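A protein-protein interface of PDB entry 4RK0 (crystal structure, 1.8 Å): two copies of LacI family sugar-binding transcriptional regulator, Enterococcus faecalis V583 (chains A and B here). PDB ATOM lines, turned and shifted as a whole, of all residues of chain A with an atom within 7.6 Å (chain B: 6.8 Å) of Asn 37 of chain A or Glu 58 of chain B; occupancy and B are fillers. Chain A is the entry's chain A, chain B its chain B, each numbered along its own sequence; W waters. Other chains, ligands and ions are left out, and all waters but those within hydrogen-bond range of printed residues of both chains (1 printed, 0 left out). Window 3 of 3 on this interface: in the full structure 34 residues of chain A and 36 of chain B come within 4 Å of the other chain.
Among the printed residues, merely in contact across the chains: Tyr 34 of chain A with Tyr 55 of chain B, Ile 39 of chain A with Tyr 55 of chain B, Asn 37 of chain A with Glu 58 of chain B, Ile 39 of chain A with Leu 59 of chain B, Ile 39 of chain A with Arg 62 of chain B and Asn 37 of chain A with Tyr 55 of chain B.
Water W1 lies within hydrogen-bond range of OH of Tyr 55 of chain B and N of Leu 40 of chain A.
Printed residues of chain A within 4 Å of Glu 58 of chain B: Asn 37.
Of the printed residues of chain B, Phe 38 of chain A touches Tyr 55 (2.8 Å).
Of the printed residues of chain B, Ile 39 of chain A touches Tyr 55 (3.4 Å), Leu 59 (3.7 Å) and Arg 62 (3.8 Å).
Of the printed residues of chain A, Tyr 55 of chain B touches Tyr 34 (3.2 Å), Asn 37 (3.98 Å), Phe 38 (2.8 Å) and Ile 39 (3.4 Å).
Of the printed residues of chain B, Tyr 34 of chain A touches Tyr 55 (3.2 Å).
Of the printed residues of chain B, Ser 7 of chain A touches Arg 62 (2.4 Å).
Glu 54 of chain B touches none of the printed residues of chain A.
The nearest printed residue of chain B that does not touch Asn 37 of chain A is Glu 54 of chain B (5.0 Å).
The nearest printed residue of chain A that does not touch Glu 58 of chain B is Lys 8 of chain A (5.9 Å).
The nearest printed residue of chain B that does not touch Tyr 34 of chain A is Leu 56 of chain B (5.3 Å).
Of the 10 printed residues of chain B, 4 touch a printed residue of chain A.
Hydrophobic or aromatic side chains of chain B within 4 Å of the printed part of chain A: Tyr 55 and Leu 59.
Printed residues of chain A that touch a printed residue of chain B: Ser 7, Tyr 34, Asn 37, Phe 38 and Ile 39.
Hydrophobic or aromatic side chains of chain A that line the printed part of chain B: Tyr 34 and Ile 39.
The backbone carbonyl oxygen of Leu 33 of chain A lies within hydrogen-bond range of the backbone NH of Phe 38 of chain A, 3.1 Å away.
OG1 of Thr 9 of chain A lies within hydrogen-bond range of OG of Ser 7 of chain A, 3.2 Å away.
The side-chain carboxylate (OE2) of Glu 58 of chain B lies within salt-bridge range of the guanidinium group (NH2) of Arg 62 of chain B (3.8 Å).
The backbone carbonyl oxygen (O) of Lys 8 of chain A is in hydrogen-bond range of the backbone NH (N) of Ile 39 of chain A, 2.9 Å away.
O of Asn 37 of chain A is in hydrogen-bond range of NH2 of Arg 62 of chain B (3.0 Å).
The backbone carbonyl oxygen of Phe 38 of chain A is in hydrogen-bond range of the side-chain hydroxyl of Tyr 55 of chain B (2.8 Å).
The guanidinium group (NH1) of Arg 62 of chain B lies within hydrogen-bond range of the backbone carbonyl oxygen (O) of Ser 7 of chain A, 2.4 Å away.
No position is printed for both chains.
Of the 9 pairs that touch across the chains among the printed residues, none has its exchanged pair printed and touching as well.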
ATOM      1  N   SER A   7       0.505  19.631  17.799  1.00  0.00           N
ATOM      2  CA  SER A   7       1.594  19.302  16.818  1.00  0.00           C
ATOM      3  C   SER A   7       2.285  17.959  17.112  1.00  0.00           C
ATOM      4  O   SER A   7       2.766  17.297  16.189  1.00  0.00           O
ATOM      5  CB  SER A   7       2.629  20.431  16.778  1.00  0.00           C
ATOM      6  OG  SER A   7       3.368  20.503  17.991  1.00  0.00           O
ATOM      7  N   LYS A   8       2.315  17.557  18.388  1.00  0.00           N
ATOM      8  CA  LYS A   8       2.948  16.299  18.826  1.00  0.00           C
ATOM      9  C   LYS A   8       4.441  16.244  18.435  1.00  0.00           C
ATOM     10  O   LYS A   8       4.911  15.302  17.812  1.00  0.00           O
ATOM     11  CB  LYS A   8       2.173  15.090  18.306  1.00  0.00           C
ATOM     12  CG  LYS A   8       0.766  14.943  18.918  1.00  0.00           C
ATOM     13  CD  LYS A   8       0.374  13.475  19.012  1.00  0.00           C
ATOM     14  CE  LYS A   8      -1.090  13.302  19.366  1.00  0.00           C
ATOM     15  NZ  LYS A   8      -1.983  13.699  18.243  1.00  0.00           N
ATOM     16  N   THR A   9       5.167  17.280  18.825  1.00  0.00           N
ATOM     17  CA  THR A   9       6.576  17.430  18.494  1.00  0.00           C
ATOM     18  C   THR A   9       7.418  17.354  19.763  1.00  0.00           C
ATOM     19  O   THR A   9       7.060  17.930  20.785  1.00  0.00           O
ATOM     20  CB  THR A   9       6.820  18.776  17.769  1.00  0.00           C
ATOM     21  OG1 THR A   9       6.393  19.864  18.603  1.00  0.00           O
ATOM     22  CG2 THR A   9       6.063  18.831  16.454  1.00  0.00           C
ATOM     23  N   VAL A  32      10.183   4.989  21.037  1.00  0.00           N
ATOM     24  CA  VAL A  32       9.025   5.302  21.878  1.00  0.00           C
ATOM     25  C   VAL A  32       8.107   6.304  21.199  1.00  0.00           C
ATOM     26  O   VAL A  32       6.886   6.068  21.080  1.00  0.00           O
ATOM     27  CB  VAL A  32       9.495   5.754  23.272  1.00  0.00           C
ATOM     28  CG1 VAL A  32       8.375   6.403  24.077  1.00  0.00           C
ATOM     29  CG2 VAL A  32      10.039   4.568  24.017  1.00  0.00           C
ATOM     30  N   LEU A  33       8.685   7.401  20.715  1.00  0.00           N
ATOM     31  CA  LEU A  33       7.941   8.434  19.991  1.00  0.00           C
ATOM     32  C   LEU A  33       7.118   7.898  18.829  1.00  0.00           C
ATOM     33  O   LEU A  33       5.971   8.295  18.685  1.00  0.00           O
ATOM     34  CB  LEU A  33       8.868   9.548  19.465  1.00  0.00           C
ATOM     35  CG  LEU A  33       9.664  10.314  20.541  1.00  0.00           C
ATOM     36  CD1 LEU A  33      10.364  11.502  19.892  1.00  0.00           C
ATOM     37  CD2 LEU A  33       8.827  10.790  21.720  1.00  0.00           C
ATOM     38  N   TYR A  34       7.698   7.028  18.005  1.00  0.00           N
ATOM     39  CA  TYR A  34       7.014   6.478  16.804  1.00  0.00           C
ATOM     40  C   TYR A  34       5.682   5.868  17.141  1.00  0.00           C
ATOM     41  O   TYR A  34       4.710   6.002  16.392  1.00  0.00           O
ATOM     42  CB  TYR A  34       7.830   5.378  16.106  1.00  0.00           C
ATOM     43  CG  TYR A  34       8.877   5.849  15.132  1.00  0.00           C
ATOM     44  CD1 TYR A  34       9.446   7.103  15.246  1.00  0.00           C
ATOM     45  CD2 TYR A  34       9.322   5.023  14.095  1.00  0.00           C
ATOM     46  CE1 TYR A  34      10.411   7.540  14.360  1.00  0.00           C
ATOM     47  CE2 TYR A  34      10.300   5.456  13.210  1.00  0.00           C
ATOM     48  CZ  TYR A  34      10.848   6.717  13.351  1.00  0.00           C
ATOM     49  OH  TYR A  34      11.824   7.175  12.481  1.00  0.00           O
ATOM     50  N   LYS A  35       5.647   5.193  18.267  1.00  0.00           N
ATOM     51  CA  LYS A  35       4.449   4.457  18.656  1.00  0.00           C
ATOM     52  C   LYS A  35       3.309   5.385  19.037  1.00  0.00           C
ATOM     53  O   LYS A  35       2.152   4.968  19.018  1.00  0.00           O
ATOM     54  CB  LYS A  35       4.759   3.490  19.784  1.00  0.00           C
ATOM     55  CG  LYS A  35       5.791   2.446  19.387  1.00  0.00           C
ATOM     56  CD  LYS A  35       5.764   1.199  20.255  1.00  0.00           C
ATOM     57  CE  LYS A  35       6.788   0.188  19.753  1.00  0.00           C
ATOM     58  NZ  LYS A  35       6.510  -1.200  20.208  1.00  0.00           N
ATOM     59  N   GLU A  36       3.617   6.647  19.337  1.00  0.00           N
ATOM     60  CA  GLU A  36       2.597   7.608  19.752  1.00  0.00           C
ATOM     61  C   GLU A  36       2.392   8.712  18.745  1.00  0.00           C
ATOM     62  O   GLU A  36       1.686   9.687  19.029  1.00  0.00           O
ATOM     63  CB  GLU A  36       3.005   8.180  21.082  1.00  0.00           C
ATOM     64  CG  GLU A  36       3.257   7.127  22.147  1.00  0.00           C
ATOM     65  CD  GLU A  36       2.185   7.100  23.213  1.00  0.00           C
ATOM     66  OE1 GLU A  36       1.940   8.159  23.829  1.00  0.00           O
ATOM     67  OE2 GLU A  36       1.606   6.019  23.445  1.00  0.00           O
ATOM     68  N   ASN A  37       3.007   8.563  17.562  1.00  0.00           N
ATOM     69  CA  ASN A  37       2.941   9.556  16.476  1.00  0.00           C
ATOM     70  C   ASN A  37       3.539  10.930  16.839  1.00  0.00           C
ATOM     71  O   ASN A  37       3.113  11.966  16.307  1.00  0.00           O
ATOM     72  CB  ASN A  37       1.507   9.702  15.926  1.00  0.00           C
ATOM     73  CG  ASN A  37       1.078   8.513  15.086  1.00  0.00           C
ATOM     74  OD1 ASN A  37      -0.063   8.066  15.183  1.00  0.00           O
ATOM     75  ND2 ASN A  37       1.990   7.992  14.255  1.00  0.00           N
ATOM     76  N   PHE A  38       4.539  10.922  17.724  1.00  0.00           N
ATOM     77  CA  PHE A  38       5.352  12.125  17.976  1.00  0.00           C
ATOM     78  C   PHE A  38       6.503  12.212  16.994  1.00  0.00           C
ATOM     79  O   PHE A  38       7.088  11.185  16.617  1.00  0.00           O
ATOM     80  CB  PHE A  38       5.877  12.131  19.403  1.00  0.00           C
ATOM     81  CG  PHE A  38       4.856  12.581  20.407  1.00  0.00           C
ATOM     82  CD1 PHE A  38       3.830  11.725  20.792  1.00  0.00           C
ATOM     83  CD2 PHE A  38       4.903  13.879  20.958  1.00  0.00           C
ATOM     84  CE1 PHE A  38       2.878  12.129  21.715  1.00  0.00           C
ATOM     85  CE2 PHE A  38       3.950  14.286  21.884  1.00  0.00           C
ATOM     86  CZ  PHE A  38       2.940  13.407  22.265  1.00  0.00           C
ATOM     87  N   ILE A  39       6.817  13.433  16.566  1.00  0.00           N
ATOM     88  CA  ILE A  39       7.951  13.654  15.685  1.00  0.00           C
ATOM     89  C   ILE A  39       9.142  14.256  16.465  1.00  0.00           C
ATOM     90  O   ILE A  39       8.963  15.023  17.408  1.00  0.00           O
ATOM     91  CB  ILE A  39       7.582  14.497  14.438  1.00  0.00           C
ATOM     92  CG1 ILE A  39       7.118  15.893  14.819  1.00  0.00           C
ATOM     93  CG2 ILE A  39       6.491  13.808  13.628  1.00  0.00           C
ATOM     94  CD1 ILE A  39       6.865  16.792  13.626  1.00  0.00           C
ATOM     95  N   LEU A  40      10.353  13.866  16.073  1.00  0.00           N
ATOM     96  CA  LEU A  40      11.573  14.218  16.784  1.00  0.00           C
ATOM     97  C   LEU A  40      12.222  15.379  16.062  1.00  0.00           C
ATOM     98  O   LEU A  40      12.550  15.275  14.886  1.00  0.00           O
ATOM     99  CB  LEU A  40      12.530  13.013  16.819  1.00  0.00           C
ATOM    100  CG  LEU A  40      13.798  13.098  17.712  1.00  0.00           C
ATOM    101  CD1 LEU A  40      14.276  11.712  18.102  1.00  0.00           C
ATOM    102  CD2 LEU A  40      14.917  13.882  17.046  1.00  0.00           C
ATOM    103  N   LEU A 245       6.906  11.695  27.788  1.00  0.00           N
ATOM    104  CA  LEU A 245       5.529  11.580  27.293  1.00  0.00           C
ATOM    105  C   LEU A 245       4.515  11.442  28.434  1.00  0.00           C
ATOM    106  O   LEU A 245       3.347  11.858  28.288  1.00  0.00           O
ATOM    107  CB  LEU A 245       5.414  10.420  26.309  1.00  0.00           C
ATOM    108  CG  LEU A 245       5.940  10.726  24.898  1.00  0.00           C
ATOM    109  CD1 LEU A 245       5.779   9.492  24.021  1.00  0.00           C
ATOM    110  CD2 LEU A 245       5.226  11.907  24.264  1.00  0.00           C
ATOM    111  N   HIS B  53       3.861   0.569   7.402  1.00  0.00           N
ATOM    112  CA  HIS B  53       4.732   1.755   7.571  1.00  0.00           C
ATOM    113  C   HIS B  53       3.892   2.993   7.956  1.00  0.00           C
ATOM    114  O   HIS B  53       3.969   4.056   7.330  1.00  0.00           O
ATOM    115  CB  HIS B  53       5.575   2.063   6.319  1.00  0.00           C
ATOM    116  CG  HIS B  53       6.747   1.148   6.102  1.00  0.00           C
ATOM    117  ND1 HIS B  53       7.512   0.634   7.130  1.00  0.00           N
ATOM    118  CD2 HIS B  53       7.316   0.703   4.955  1.00  0.00           C
ATOM    119  CE1 HIS B  53       8.482  -0.111   6.624  1.00  0.00           C
ATOM    120  NE2 HIS B  53       8.379  -0.092   5.308  1.00  0.00           N
ATOM    121  N   GLU B  54       3.108   2.838   9.012  1.00  0.00           N
ATOM    122  CA  GLU B  54       2.116   3.842   9.401  1.00  0.00           C
ATOM    123  C   GLU B  54       2.778   5.132   9.850  1.00  0.00           C
ATOM    124  O   GLU B  54       2.204   6.209   9.636  1.00  0.00           O
ATOM    125  CB  GLU B  54       1.205   3.311  10.519  1.00  0.00           C
ATOM    126  CG  GLU B  54       0.479   2.022  10.138  1.00  0.00           C
ATOM    127  CD  GLU B  54      -0.391   1.465  11.242  1.00  0.00           C
ATOM    128  OE1 GLU B  54      -0.120   1.755  12.430  1.00  0.00           O
ATOM    129  OE2 GLU B  54      -1.343   0.722  10.908  1.00  0.00           O
ATOM    130  N   TYR B  55       3.986   5.039  10.433  1.00  0.00           N
ATOM    131  CA  TYR B  55       4.715   6.239  10.901  1.00  0.00           C
ATOM    132  C   TYR B  55       5.200   7.043   9.724  1.00  0.00           C
ATOM    133  O   TYR B  55       5.080   8.261   9.708  1.00  0.00           O
ATOM    134  CB  TYR B  55       5.916   5.897  11.793  1.00  0.00           C
ATOM    135  CG  TYR B  55       6.530   7.137  12.411  1.00  0.00           C
ATOM    136  CD1 TYR B  55       5.883   7.806  13.439  1.00  0.00           C
ATOM    137  CD2 TYR B  55       7.701   7.688  11.912  1.00  0.00           C
ATOM    138  CE1 TYR B  55       6.415   8.962  13.988  1.00  0.00           C
ATOM    139  CE2 TYR B  55       8.254   8.849  12.460  1.00  0.00           C
ATOM    140  CZ  TYR B  55       7.610   9.478  13.500  1.00  0.00           C
ATOM    141  OH  TYR B  55       8.138  10.641  14.052  1.00  0.00           O
ATOM    142  N   LEU B  56       5.762   6.366   8.730  1.00  0.00           N
ATOM    143  CA  LEU B  56       6.218   7.062   7.520  1.00  0.00           C
ATOM    144  C   LEU B  56       5.048   7.758   6.794  1.00  0.00           C
ATOM    145  O   LEU B  56       5.213   8.863   6.299  1.00  0.00           O
ATOM    146  CB  LEU B  56       6.970   6.097   6.572  1.00  0.00           C
ATOM    147  CG  LEU B  56       8.186   5.365   7.170  1.00  0.00           C
ATOM    148  CD1 LEU B  56       8.992   4.665   6.087  1.00  0.00           C
ATOM    149  CD2 LEU B  56       9.085   6.270   8.009  1.00  0.00           C
ATOM    150  N   THR B  57       3.893   7.109   6.729  1.00  0.00           N
ATOM    151  CA  THR B  57       2.683   7.737   6.171  1.00  0.00           C
ATOM    152  C   THR B  57       2.279   8.951   7.025  1.00  0.00           C
ATOM    153  O   THR B  57       2.110  10.062   6.511  1.00  0.00           O
ATOM    154  CB  THR B  57       1.536   6.717   6.073  1.00  0.00           C
ATOM    155  OG1 THR B  57       1.967   5.619   5.265  1.00  0.00           O
ATOM    156  CG2 THR B  57       0.293   7.335   5.441  1.00  0.00           C
ATOM    157  N   GLU B  58       2.162   8.758   8.331  1.00  0.00           N
ATOM    158  CA  GLU B  58       1.838   9.865   9.229  1.00  0.00           C
ATOM    159  C   GLU B  58       2.782  11.040   8.943  1.00  0.00           C
ATOM    160  O   GLU B  58       2.336  12.175   8.765  1.00  0.00           O
ATOM    161  CB  GLU B  58       1.938   9.432  10.690  1.00  0.00           C
ATOM    162  CG  GLU B  58       1.883  10.569  11.716  1.00  0.00           C
ATOM    163  CD  GLU B  58       0.475  10.948  12.158  1.00  0.00           C
ATOM    164  OE1 GLU B  58      -0.507  10.653  11.439  1.00  0.00           O
ATOM    165  OE2 GLU B  58       0.352  11.559  13.242  1.00  0.00           O
ATOM    166  N   LEU B  59       4.081  10.758   8.855  1.00  0.00           N
ATOM    167  CA  LEU B  59       5.100  11.832   8.787  1.00  0.00           C
ATOM    168  C   LEU B  59       5.053  12.564   7.461  1.00  0.00           C
ATOM    169  O   LEU B  59       5.104  13.803   7.413  1.00  0.00           O
ATOM    170  CB  LEU B  59       6.504  11.274   8.997  1.00  0.00           C
ATOM    171  CG  LEU B  59       7.634  12.322   8.972  1.00  0.00           C
ATOM    172  CD1 LEU B  59       7.938  12.790  10.386  1.00  0.00           C
ATOM    173  CD2 LEU B  59       8.886  11.750   8.332  1.00  0.00           C
ATOM    174  N   ILE B  60       4.940  11.798   6.387  1.00  0.00           N
ATOM    175  CA  ILE B  60       4.963  12.347   5.044  1.00  0.00           C
ATOM    176  C   ILE B  60       3.732  13.203   4.749  1.00  0.00           C
ATOM    177  O   ILE B  60       3.742  14.030   3.843  1.00  0.00           O
ATOM    178  CB  ILE B  60       5.158  11.255   3.981  1.00  0.00           C
ATOM    179  CG1 ILE B  60       6.078  11.804   2.878  1.00  0.00           C
ATOM    180  CG2 ILE B  60       3.816  10.702   3.510  1.00  0.00           C
ATOM    181  CD1 ILE B  60       5.850  11.233   1.502  1.00  0.00           C
ATOM    182  N   ARG B  61       2.690  13.017   5.537  1.00  0.00           N
ATOM    183  CA  ARG B  61       1.515  13.847   5.433  1.00  0.00           C
ATOM    184  C   ARG B  61       1.582  15.143   6.232  1.00  0.00           C
ATOM    185  O   ARG B  61       0.643  15.908   6.205  1.00  0.00           O
ATOM    186  CB  ARG B  61       0.322  13.033   5.889  1.00  0.00           C
ATOM    187  CG  ARG B  61       0.029  11.941   4.915  1.00  0.00           C
ATOM    188  CD  ARG B  61      -1.188  11.147   5.317  1.00  0.00           C
ATOM    189  NE  ARG B  61      -1.502  10.231   4.217  1.00  0.00           N
ATOM    190  CZ  ARG B  61      -2.407   9.264   4.276  1.00  0.00           C
ATOM    191  NH1 ARG B  61      -3.118   9.069   5.382  1.00  0.00           N
ATOM    192  NH2 ARG B  61      -2.593   8.484   3.223  1.00  0.00           N
ATOM    193  N   ARG B  62       2.665  15.375   6.963  1.00  0.00           N
ATOM    194  CA  ARG B  62       2.789  16.571   7.759  1.00  0.00           C
ATOM    195  C   ARG B  62       3.035  17.786   6.858  1.00  0.00           C
ATOM    196  O   ARG B  62       3.700  17.679   5.813  1.00  0.00           O
ATOM    197  CB  ARG B  62       3.933  16.452   8.767  1.00  0.00           C
ATOM    198  CG  ARG B  62       3.717  15.406   9.845  1.00  0.00           C
ATOM    199  CD  ARG B  62       3.068  15.986  11.088  1.00  0.00           C
ATOM    200  NE  ARG B  62       2.959  14.972  12.133  1.00  0.00           N
ATOM    201  CZ  ARG B  62       2.889  15.223  13.440  1.00  0.00           C
ATOM    202  NH1 ARG B  62       2.917  16.471  13.897  1.00  0.00           N
ATOM    203  NH2 ARG B  62       2.800  14.210  14.297  1.00  0.00           N
HETATM  204  O   HOH W   1      10.518  11.632  14.310  1.00  0.00           O
